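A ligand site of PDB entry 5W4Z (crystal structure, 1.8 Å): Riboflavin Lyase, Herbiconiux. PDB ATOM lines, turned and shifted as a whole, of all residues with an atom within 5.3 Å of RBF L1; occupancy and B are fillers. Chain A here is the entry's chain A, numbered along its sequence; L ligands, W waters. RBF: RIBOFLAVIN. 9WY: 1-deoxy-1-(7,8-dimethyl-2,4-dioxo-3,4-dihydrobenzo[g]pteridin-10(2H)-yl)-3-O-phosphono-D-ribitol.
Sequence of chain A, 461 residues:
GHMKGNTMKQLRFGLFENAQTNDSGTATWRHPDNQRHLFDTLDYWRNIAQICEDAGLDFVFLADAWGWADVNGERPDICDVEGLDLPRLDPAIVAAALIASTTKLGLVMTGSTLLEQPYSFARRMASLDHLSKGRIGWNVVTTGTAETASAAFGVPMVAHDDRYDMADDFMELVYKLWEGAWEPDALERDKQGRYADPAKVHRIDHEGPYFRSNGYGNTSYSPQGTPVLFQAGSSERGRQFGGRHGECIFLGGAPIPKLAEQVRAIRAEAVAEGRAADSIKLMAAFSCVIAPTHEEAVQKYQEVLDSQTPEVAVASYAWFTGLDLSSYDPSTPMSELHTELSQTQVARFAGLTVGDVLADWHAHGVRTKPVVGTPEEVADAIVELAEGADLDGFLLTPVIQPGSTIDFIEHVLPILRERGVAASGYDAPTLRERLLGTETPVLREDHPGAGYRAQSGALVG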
ATOM      1  N   PHE A  16      14.764   2.307  -7.229  1.00  0.00           N
ATOM      2  CA  PHE A  16      15.385   2.676  -5.963  1.00  0.00           C
ATOM      3  C   PHE A  16      16.905   2.556  -6.042  1.00  0.00           C
ATOM      4  O   PHE A  16      17.425   1.536  -6.506  1.00  0.00           O
ATOM      5  CB  PHE A  16      14.843   1.777  -4.846  1.00  0.00           C
ATOM      6  CG  PHE A  16      15.515   1.984  -3.500  1.00  0.00           C
ATOM      7  CD1 PHE A  16      15.074   2.966  -2.629  1.00  0.00           C
ATOM      8  CD2 PHE A  16      16.587   1.183  -3.126  1.00  0.00           C
ATOM      9  CE1 PHE A  16      15.689   3.147  -1.407  1.00  0.00           C
ATOM     10  CE2 PHE A  16      17.202   1.364  -1.904  1.00  0.00           C
ATOM     11  CZ  PHE A  16      16.759   2.353  -1.040  1.00  0.00           C
ATOM     12  N   ASN A  18      20.849   4.247  -4.048  1.00  0.00           N
ATOM     13  CA  ASN A  18      21.418   5.145  -3.045  1.00  0.00           C
ATOM     14  C   ASN A  18      22.899   5.359  -3.326  1.00  0.00           C
ATOM     15  O   ASN A  18      23.566   4.502  -3.894  1.00  0.00           O
ATOM     16  CB  ASN A  18      21.174   4.636  -1.596  1.00  0.00           C
ATOM     17  CG  ASN A  18      21.809   3.275  -1.269  1.00  0.00           C
ATOM     18  OD1 ASN A  18      21.459   2.690  -0.246  1.00  0.00           O
ATOM     19  ND2 ASN A  18      22.740   2.795  -2.097  1.00  0.00           N
ATOM     20  N   GLN A  20      25.826   5.044  -2.221  1.00  0.00           N
ATOM     21  CA  GLN A  20      26.822   4.306  -1.460  1.00  0.00           C
ATOM     22  C   GLN A  20      26.859   2.880  -2.003  1.00  0.00           C
ATOM     23  O   GLN A  20      26.031   2.496  -2.830  1.00  0.00           O
ATOM     24  CB  GLN A  20      26.534   4.337   0.045  1.00  0.00           C
ATOM     25  CG  GLN A  20      25.189   3.750   0.487  1.00  0.00           C
ATOM     26  CD  GLN A  20      24.958   3.941   1.976  1.00  0.00           C
ATOM     27  OE1 GLN A  20      24.588   5.025   2.425  1.00  0.00           O
ATOM     28  NE2 GLN A  20      25.210   2.898   2.762  1.00  0.00           N
ATOM     29  N   ASN A  22      26.534  -0.331  -0.751  1.00  0.00           N
ATOM     30  CA  ASN A  22      25.499  -1.281  -0.377  1.00  0.00           C
ATOM     31  C   ASN A  22      24.229  -0.509  -0.019  1.00  0.00           C
ATOM     32  O   ASN A  22      24.214   0.718   0.015  1.00  0.00           O
ATOM     33  CB  ASN A  22      25.990  -2.160   0.765  1.00  0.00           C
ATOM     34  CG  ASN A  22      27.170  -3.035   0.345  1.00  0.00           C
ATOM     35  OD1 ASN A  22      27.059  -3.804  -0.606  1.00  0.00           O
ATOM     36  ND2 ASN A  22      28.299  -2.897   1.036  1.00  0.00           N
ATOM     37  N   ASP A  23      23.140  -1.244   0.226  1.00  0.00           N
ATOM     38  CA  ASP A  23      21.887  -0.562   0.544  1.00  0.00           C
ATOM     39  C   ASP A  23      21.093  -1.368   1.562  1.00  0.00           C
ATOM     40  O   ASP A  23      21.230  -2.592   1.668  1.00  0.00           O
ATOM     41  CB  ASP A  23      21.041  -0.333  -0.720  1.00  0.00           C
ATOM     42  CG  ASP A  23      20.424  -1.610  -1.242  1.00  0.00           C
ATOM     43  OD1 ASP A  23      21.115  -2.340  -1.966  1.00  0.00           O
ATOM     44  OD2 ASP A  23      19.222  -1.868  -0.938  1.00  0.00           O
ATOM     45  N   SER A  24      20.268  -0.652   2.317  1.00  0.00           N
ATOM     46  CA  SER A  24      19.194  -1.236   3.113  1.00  0.00           C
ATOM     47  C   SER A  24      19.692  -2.142   4.225  1.00  0.00           C
ATOM     48  O   SER A  24      18.940  -2.957   4.760  1.00  0.00           O
ATOM     49  CB  SER A  24      18.222  -1.999   2.209  1.00  0.00           C
ATOM     50  OG  SER A  24      17.715  -1.152   1.188  1.00  0.00           O
ATOM     51  N   GLY A  25      20.965  -2.007   4.613  1.00  0.00           N
ATOM     52  CA  GLY A  25      21.513  -2.839   5.650  1.00  0.00           C
ATOM     53  C   GLY A  25      22.005  -4.196   5.202  1.00  0.00           C
ATOM     54  O   GLY A  25      22.444  -4.984   6.041  1.00  0.00           O
ATOM     55  N   ALA A  63      17.773   7.161  -2.041  1.00  0.00           N
ATOM     56  CA  ALA A  63      17.585   7.196  -0.595  1.00  0.00           C
ATOM     57  C   ALA A  63      18.693   8.035   0.031  1.00  0.00           C
ATOM     58  O   ALA A  63      19.605   8.505  -0.650  1.00  0.00           O
ATOM     59  CB  ALA A  63      17.577   5.777  -0.020  1.00  0.00           C
ATOM     60  N   ASP A  64      18.637   8.234   1.350  1.00  0.00           N
ATOM     61  CA  ASP A  64      19.734   8.913   2.021  1.00  0.00           C
ATOM     62  C   ASP A  64      19.831   8.421   3.461  1.00  0.00           C
ATOM     63  O   ASP A  64      18.882   7.855   4.010  1.00  0.00           O
ATOM     64  CB  ASP A  64      19.549  10.435   1.974  1.00  0.00           C
ATOM     65  CG  ASP A  64      20.817  11.226   2.362  1.00  0.00           C
ATOM     66  OD1 ASP A  64      21.947  10.686   2.218  1.00  0.00           O
ATOM     67  OD2 ASP A  64      20.668  12.386   2.801  1.00  0.00           O
ATOM     68  N   ALA A  65      21.004   8.621   4.039  1.00  0.00           N
ATOM     69  CA  ALA A  65      21.229   8.397   5.461  1.00  0.00           C
ATOM     70  C   ALA A  65      22.266   9.408   5.918  1.00  0.00           C
ATOM     71  O   ALA A  65      23.151   9.807   5.159  1.00  0.00           O
ATOM     72  CB  ALA A  65      21.700   6.961   5.752  1.00  0.00           C
ATOM     73  N   THR A 143      14.567  10.899   9.147  1.00  0.00           N
ATOM     74  CA  THR A 143      15.886  10.327   9.438  1.00  0.00           C
ATOM     75  C   THR A 143      15.826   9.141  10.389  1.00  0.00           C
ATOM     76  O   THR A 143      15.578   9.298  11.597  1.00  0.00           O
ATOM     77  CB  THR A 143      16.843  11.395   9.952  1.00  0.00           C
ATOM     78  OG1 THR A 143      17.030  12.364   8.925  1.00  0.00           O
ATOM     79  CG2 THR A 143      18.225  10.796  10.327  1.00  0.00           C
ATOM     80  N   GLY A 144      16.064   7.939   9.862  1.00  0.00           N
ATOM     81  CA  GLY A 144      16.045   6.714  10.656  1.00  0.00           C
ATOM     82  C   GLY A 144      17.312   6.438  11.419  1.00  0.00           C
ATOM     83  O   GLY A 144      17.358   5.499  12.221  1.00  0.00           O
ATOM     84  N   THR A 145      18.348   7.230  11.178  1.00  0.00           N
ATOM     85  CA  THR A 145      19.624   7.141  11.864  1.00  0.00           C
ATOM     86  C   THR A 145      19.811   8.328  12.794  1.00  0.00           C
ATOM     87  O   THR A 145      20.906   8.890  12.915  1.00  0.00           O
ATOM     88  CB  THR A 145      20.757   7.055  10.843  1.00  0.00           C
ATOM     89  OG1 THR A 145      20.739   8.227  10.022  1.00  0.00           O
ATOM     90  CG2 THR A 145      20.584   5.827   9.971  1.00  0.00           C
ATOM     91  N   PHE A 250       5.904   5.877  -0.491  1.00  0.00           N
ATOM     92  CA  PHE A 250       6.774   4.728  -0.676  1.00  0.00           C
ATOM     93  C   PHE A 250       6.520   3.755   0.474  1.00  0.00           C
ATOM     94  O   PHE A 250       6.755   4.095   1.634  1.00  0.00           O
ATOM     95  CB  PHE A 250       8.226   5.233  -0.705  1.00  0.00           C
ATOM     96  CG  PHE A 250       9.240   4.209  -1.163  1.00  0.00           C
ATOM     97  CD1 PHE A 250       8.861   3.017  -1.766  1.00  0.00           C
ATOM     98  CD2 PHE A 250      10.611   4.462  -0.983  1.00  0.00           C
ATOM     99  CE1 PHE A 250       9.817   2.102  -2.181  1.00  0.00           C
ATOM    100  CE2 PHE A 250      11.569   3.540  -1.391  1.00  0.00           C
ATOM    101  CZ  PHE A 250      11.166   2.353  -1.994  1.00  0.00           C
ATOM    102  N   LEU A 251       6.019   2.564   0.150  1.00  0.00           N
ATOM    103  CA  LEU A 251       5.741   1.524   1.135  1.00  0.00           C
ATOM    104  C   LEU A 251       6.695   0.343   0.977  1.00  0.00           C
ATOM    105  O   LEU A 251       7.016  -0.057  -0.152  1.00  0.00           O
ATOM    106  CB  LEU A 251       4.306   1.015   1.007  1.00  0.00           C
ATOM    107  CG  LEU A 251       3.207   1.997   1.436  1.00  0.00           C
ATOM    108  CD1 LEU A 251       1.835   1.385   1.193  1.00  0.00           C
ATOM    109  CD2 LEU A 251       3.375   2.359   2.907  1.00  0.00           C
ATOM    110  N   GLY A 252       7.121  -0.236   2.097  1.00  0.00           N
ATOM    111  CA  GLY A 252       7.867  -1.469   2.046  1.00  0.00           C
ATOM    112  C   GLY A 252       6.999  -2.633   1.580  1.00  0.00           C
ATOM    113  O   GLY A 252       5.769  -2.561   1.554  1.00  0.00           O
ATOM    114  N   GLY A 253       7.654  -3.726   1.201  1.00  0.00           N
ATOM    115  CA  GLY A 253       6.897  -4.909   0.795  1.00  0.00           C
ATOM    116  C   GLY A 253       6.210  -5.580   1.975  1.00  0.00           C
ATOM    117  O   GLY A 253       6.673  -5.520   3.109  1.00  0.00           O
ATOM    118  N   ALA A 285       7.808  -1.054  -2.681  1.00  0.00           N
ATOM    119  CA  ALA A 285       9.112  -1.614  -3.039  1.00  0.00           C
ATOM    120  C   ALA A 285       8.903  -3.008  -3.627  1.00  0.00           C
ATOM    121  O   ALA A 285       7.987  -3.734  -3.225  1.00  0.00           O
ATOM    122  CB  ALA A 285      10.015  -1.688  -1.824  1.00  0.00           C
ATOM    123  N   TRP A 319      22.124  -0.077  13.125  1.00  0.00           N
ATOM    124  CA  TRP A 319      22.182   1.110  12.279  1.00  0.00           C
ATOM    125  C   TRP A 319      20.824   1.792  12.189  1.00  0.00           C
ATOM    126  O   TRP A 319      20.738   3.032  12.186  1.00  0.00           O
ATOM    127  CB  TRP A 319      22.688   0.697  10.895  1.00  0.00           C
ATOM    128  CG  TRP A 319      22.832   1.785   9.858  1.00  0.00           C
ATOM    129  CD1 TRP A 319      22.841   3.133  10.067  1.00  0.00           C
ATOM    130  CD2 TRP A 319      22.978   1.596   8.444  1.00  0.00           C
ATOM    131  NE1 TRP A 319      22.996   3.807   8.864  1.00  0.00           N
ATOM    132  CE2 TRP A 319      23.078   2.873   7.853  1.00  0.00           C
ATOM    133  CE3 TRP A 319      23.050   0.469   7.622  1.00  0.00           C
ATOM    134  CZ2 TRP A 319      23.228   3.056   6.483  1.00  0.00           C
ATOM    135  CZ3 TRP A 319      23.200   0.652   6.252  1.00  0.00           C
ATOM    136  CH2 TRP A 319      23.287   1.929   5.696  1.00  0.00           C
ATOM    137  N   PHE A 320      19.743   1.018  12.154  1.00  0.00           N
ATOM    138  CA  PHE A 320      18.421   1.588  11.951  1.00  0.00           C
ATOM    139  C   PHE A 320      17.626   1.735  13.232  1.00  0.00           C
ATOM    140  O   PHE A 320      16.717   2.568  13.278  1.00  0.00           O
ATOM    141  CB  PHE A 320      17.646   0.739  10.936  1.00  0.00           C
ATOM    142  CG  PHE A 320      18.301   0.684   9.591  1.00  0.00           C
ATOM    143  CD1 PHE A 320      18.238   1.773   8.729  1.00  0.00           C
ATOM    144  CD2 PHE A 320      19.029  -0.436   9.204  1.00  0.00           C
ATOM    145  CE1 PHE A 320      18.864   1.733   7.498  1.00  0.00           C
ATOM    146  CE2 PHE A 320      19.649  -0.483   7.969  1.00  0.00           C
ATOM    147  CZ  PHE A 320      19.565   0.605   7.113  1.00  0.00           C
ATOM    148  N   SER A 342      14.024   4.007  13.642  1.00  0.00           N
ATOM    149  CA  SER A 342      13.194   3.395  12.595  1.00  0.00           C
ATOM    150  C   SER A 342      12.232   2.406  13.259  1.00  0.00           C
ATOM    151  O   SER A 342      12.521   1.223  13.400  1.00  0.00           O
ATOM    152  CB  SER A 342      14.071   2.715  11.549  1.00  0.00           C
ATOM    153  OG  SER A 342      15.101   3.595  11.075  1.00  0.00           O
ATOM    154  N   GLN A 345      11.077  -0.981  11.623  1.00  0.00           N
ATOM    155  CA  GLN A 345      12.003  -2.108  11.709  1.00  0.00           C
ATOM    156  C   GLN A 345      11.906  -2.861  13.033  1.00  0.00           C
ATOM    157  O   GLN A 345      12.539  -3.909  13.167  1.00  0.00           O
ATOM    158  CB  GLN A 345      13.437  -1.646  11.494  1.00  0.00           C
ATOM    159  CG  GLN A 345      13.643  -0.987  10.153  1.00  0.00           C
ATOM    160  CD  GLN A 345      13.057  -1.816   9.035  1.00  0.00           C
ATOM    161  OE1 GLN A 345      13.217  -3.034   9.006  1.00  0.00           O
ATOM    162  NE2 GLN A 345      12.372  -1.155   8.103  1.00  0.00           N
ATOM    163  N   VAL A 366      16.286  -3.936   5.727  1.00  0.00           N
ATOM    164  CA  VAL A 366      14.998  -3.242   5.805  1.00  0.00           C
ATOM    165  C   VAL A 366      14.047  -3.600   4.677  1.00  0.00           C
ATOM    166  O   VAL A 366      12.888  -3.180   4.692  1.00  0.00           O
ATOM    167  CB  VAL A 366      15.169  -1.716   5.833  1.00  0.00           C
ATOM    168  CG1 VAL A 366      16.020  -1.311   7.013  1.00  0.00           C
ATOM    169  CG2 VAL A 366      15.793  -1.250   4.535  1.00  0.00           C
ATOM    170  N   ARG A 367      14.504  -4.373   3.691  1.00  0.00           N
ATOM    171  CA  ARG A 367      13.642  -4.779   2.587  1.00  0.00           C
ATOM    172  C   ARG A 367      12.983  -6.125   2.897  1.00  0.00           C
ATOM    173  O   ARG A 367      13.031  -6.616   4.028  1.00  0.00           O
ATOM    174  CB  ARG A 367      14.430  -4.832   1.289  1.00  0.00           C
ATOM    175  CG  ARG A 367      14.906  -3.482   0.839  1.00  0.00           C
ATOM    176  CD  ARG A 367      16.173  -3.643   0.049  1.00  0.00           C
ATOM    177  NE  ARG A 367      16.029  -4.571  -1.055  1.00  0.00           N
ATOM    178  CZ  ARG A 367      17.041  -4.965  -1.807  1.00  0.00           C
ATOM    179  NH1 ARG A 367      18.261  -4.513  -1.561  1.00  0.00           N
ATOM    180  NH2 ARG A 367      16.844  -5.822  -2.805  1.00  0.00           N
ATOM    181  N   THR A 397      13.694  -2.450  -6.334  1.00  0.00           N
ATOM    182  CA  THR A 397      14.807  -2.399  -5.387  1.00  0.00           C
ATOM    183  C   THR A 397      15.818  -3.452  -5.801  1.00  0.00           C
ATOM    184  O   THR A 397      15.621  -4.649  -5.553  1.00  0.00           O
ATOM    185  CB  THR A 397      14.339  -2.619  -3.948  1.00  0.00           C
ATOM    186  OG1 THR A 397      13.553  -3.810  -3.863  1.00  0.00           O
ATOM    187  CG2 THR A 397      13.512  -1.430  -3.500  1.00  0.00           C
HETATM  188  N1  RBF L   1      16.049   3.653   5.917  1.00  0.00           N
HETATM  189  C2  RBF L   1      15.914   3.922   7.232  1.00  0.00           C
HETATM  190  O2  RBF L   1      16.657   4.685   7.770  1.00  0.00           O
HETATM  191  N3  RBF L   1      14.928   3.329   7.959  1.00  0.00           N
HETATM  192  C4  RBF L   1      14.085   2.495   7.367  1.00  0.00           C
HETATM  193  O4  RBF L   1      13.241   1.988   8.001  1.00  0.00           O
HETATM  194  C4A RBF L   1      14.201   2.211   6.013  1.00  0.00           C
HETATM  195  N5  RBF L   1      13.317   1.340   5.397  1.00  0.00           N
HETATM  196  C5A RBF L   1      13.441   1.060   4.088  1.00  0.00           C
HETATM  197  C6  RBF L   1      12.538   0.147   3.449  1.00  0.00           C
HETATM  198  C7  RBF L   1      12.676  -0.136   2.089  1.00  0.00           C
HETATM  199  C7M RBF L   1      11.691  -1.087   1.512  1.00  0.00           C
HETATM  200  C8  RBF L   1      13.702   0.468   1.360  1.00  0.00           C
HETATM  201  C8M RBF L   1      13.920   0.221  -0.139  1.00  0.00           C
HETATM  202  C9  RBF L   1      14.586   1.369   1.978  1.00  0.00           C
HETATM  203  C9A RBF L   1      14.450   1.647   3.362  1.00  0.00           C
HETATM  204  N10 RBF L   1      15.302   2.499   3.940  1.00  0.00           N
HETATM  205  C10 RBF L   1      15.184   2.790   5.288  1.00  0.00           C
HETATM  206  C1' RBF L   1      16.434   3.241   3.333  1.00  0.00           C
HETATM  207  C2' RBF L   1      17.682   2.320   3.198  1.00  0.00           C
HETATM  208  O2' RBF L   1      18.099   1.917   4.457  1.00  0.00           O
HETATM  209  C3' RBF L   1      18.818   3.107   2.503  1.00  0.00           C
HETATM  210  O3' RBF L   1      19.579   2.206   1.726  1.00  0.00           O
HETATM  211  C4' RBF L   1      19.676   3.798   3.533  1.00  0.00           C
HETATM  212  O4' RBF L   1      18.969   4.876   4.136  1.00  0.00           O
HETATM  213  C5' RBF L   1      20.938   4.409   2.850  1.00  0.00           C
HETATM  214  O5' RBF L   1      20.531   5.401   1.885  1.00  0.00           O
HETATM  215  C10 9WY L   2      13.597   6.357   5.423  1.00  0.00           C
HETATM  216  C7  9WY L   2      10.818   3.244   2.745  1.00  0.00           C
HETATM  217  O3P 9WY L   2       7.759   5.973  10.293  1.00  0.00           O
HETATM  218  P   9WY L   2       9.037   5.313  10.403  1.00  0.00           P
HETATM  219  O1P 9WY L   2       9.434   5.480  11.773  1.00  0.00           O
HETATM  220  O2P 9WY L   2       8.941   3.912  10.020  1.00  0.00           O
HETATM  221  O5' 9WY L   2      12.584   8.728  11.433  1.00  0.00           O
HETATM  222  C5' 9WY L   2      11.898   7.539  11.115  1.00  0.00           C
HETATM  223  C4' 9WY L   2      11.999   7.245   9.652  1.00  0.00           C
HETATM  224  O4' 9WY L   2      13.365   7.283   9.272  1.00  0.00           O
HETATM  225  C3' 9WY L   2      11.442   5.855   9.437  1.00  0.00           C
HETATM  226  O3' 9WY L   2      10.027   5.972   9.359  1.00  0.00           O
HETATM  227  C2' 9WY L   2      12.046   5.202   8.201  1.00  0.00           C
HETATM  228  O2' 9WY L   2      11.364   3.993   8.009  1.00  0.00           O
HETATM  229  C1' 9WY L   2      11.777   6.040   7.000  1.00  0.00           C
HETATM  230  N10 9WY L   2      12.419   5.735   5.741  1.00  0.00           N
HETATM  231  C9A 9WY L   2      11.865   4.916   4.756  1.00  0.00           C
HETATM  232  C9  9WY L   2      10.671   4.265   4.991  1.00  0.00           C
HETATM  233  C8  9WY L   2      10.135   3.439   4.036  1.00  0.00           C
HETATM  234  C8M 9WY L   2       8.836   2.772   4.290  1.00  0.00           C
HETATM  235  C7M 9WY L   2      10.223   2.354   1.700  1.00  0.00           C
HETATM  236  C6  9WY L   2      12.014   3.889   2.517  1.00  0.00           C
HETATM  237  C5A 9WY L   2      12.552   4.708   3.479  1.00  0.00           C
HETATM  238  N5  9WY L   2      13.713   5.321   3.232  1.00  0.00           N
HETATM  239  N1  9WY L   2      14.194   7.164   6.293  1.00  0.00           N
HETATM  240  C4A 9WY L   2      14.242   6.114   4.139  1.00  0.00           C
HETATM  241  C4  9WY L   2      15.511   6.814   3.915  1.00  0.00           C
HETATM  242  O4  9WY L   2      16.104   6.681   2.866  1.00  0.00           O
HETATM  243  N3  9WY L   2      15.993   7.571   4.861  1.00  0.00           N
HETATM  244  C2  9WY L   2      15.377   7.744   6.004  1.00  0.00           C
HETATM  245  O2  9WY L   2      15.896   8.484   6.830  1.00  0.00           O
HETATM  246  O   HOH W   1      22.800   6.704   0.985  1.00  0.00           O
HETATM  247  O   HOH W   2      18.775   5.529   6.786  1.00  0.00           O
HETATM  248  O   HOH W   3      11.306   2.186  10.255  1.00  0.00           O
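An oxygen (O4) of RBF L1 lies within hydrogen-bond range of an oxygen (O2') of 9WY L2 (2.7 Å).
O4' of 9WY L2 sits at hydrogen-bond distance from N of Gly 144. The side-chain amide oxygen (OD1) of Asn 18 lies within hydrogen-bond range of an oxygen (O3') of RBF L1, 2.8 Å away. NE2 of Gln 345 lies within hydrogen-bond range of O4 of RBF L1. The backbone carbonyl oxygen of Asp 64 is in hydrogen-bond range of an oxygen (O4') of RBF L1. The backbone carbonyl oxygen (O) of Asp 64 lies within hydrogen-bond range of a nitrogen (N3) of 9WY L2 (3.0 Å). An oxygen (O4) of 9WY L2 lies within hydrogen-bond range of the backbone NH (N) of Asp 64 (3.3 Å). O of Thr 143 sits at hydrogen-bond distance from O5' of 9WY L2 (3.1 Å). The backbone NH (N) of Ser 24 sits at hydrogen-bond distance from an oxygen (O3') of RBF L1 (3.0 Å). A nitrogen (N3) of RBF L1 sits at hydrogen-bond distance from the side-chain hydroxyl of Ser 342 (3.1 Å). N of Asp 64 lies within hydrogen-bond range of O5' of RBF L1, at 3.4 Å.
N of Val 366 lies within hydrogen-bond range of O of Ser 24, at 3.0 Å. The backbone carbonyl oxygen of Asn 22 sits at hydrogen-bond distance from the side-chain amide nitrogen of Asn 18, at 3.3 Å. OD2 of Asp 23 lies within hydrogen-bond range of OG of Ser 24 (2.7 Å). N of Ala 285 lies within hydrogen-bond range of O of Leu 251 (2.8 Å). The backbone carbonyl oxygen (O) of Thr 397 is in hydrogen-bond range of the guanidinium group (NH2) of Arg 367 (3.2 Å). OG of Ser 342 lies within hydrogen-bond range of O of Phe 320. The side-chain carboxylate of Asp 23 lies within salt-bridge range of the guanidinium group of Arg 367 (2.9 Å). ND2 of Asn 18 sits at hydrogen-bond distance from O of Gln 20, at 3.4 Å.
Water W1 bridges an oxygen (O5') of RBF L1 and the side-chain amide oxygen (OE1) of Gln 20. Water W3 lies within hydrogen-bond range of O2' of 9WY L2 (2.9 Å), O4 of RBF L1 (3.0 Å) and N of Gln 345 (3.5 Å).
Phe 16 touches RBF L1 (CE1 to C8M, 3.6 Å). OE1 of Gln 20 touches C5' of RBF L1, at 3.7 Å. Asp 23 touches RBF L1. Ala 63 touches RBF L1. Ala 65 touches RBF L1 (CB to O4', 3.8 Å). Gly 144 touches RBF L1. Phe 250 touches RBF L1 (CZ to C8M, 3.9 Å). CA of Gly 252 touches C7M of RBF L1, 3.9 Å away. Ala 285 touches RBF L1 (CB to C7M, 3.8 Å). Phe 320 touches RBF L1 (CE1 to O2', 3.1 Å). Val 366 touches RBF L1 (CG2 to C5A, 3.3 Å). Arg 367 touches RBF L1. Thr 397 touches RBF L1 (CG2 to C8M, 3.8 Å). Hydrophobic or aromatic side chains within 4 Å of RBF L1: Phe 16, Ala 63, Ala 65, Phe 250, Ala 285, Phe 320 and Val 366. Within 4 Å of RBF L1: Phe 16, Asn 18, Gln 20, Asp 23, Ser 24, Ala 63, Asp 64, Ala 65, Gly 144, Phe 250, Gly 252, Ala 285, Phe 320, Ser 342, Gln 345, Val 366, Arg 367 and Thr 397. The nearest printed residue that does not touch RBF L1 is Trp 319 (4.4 Å).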
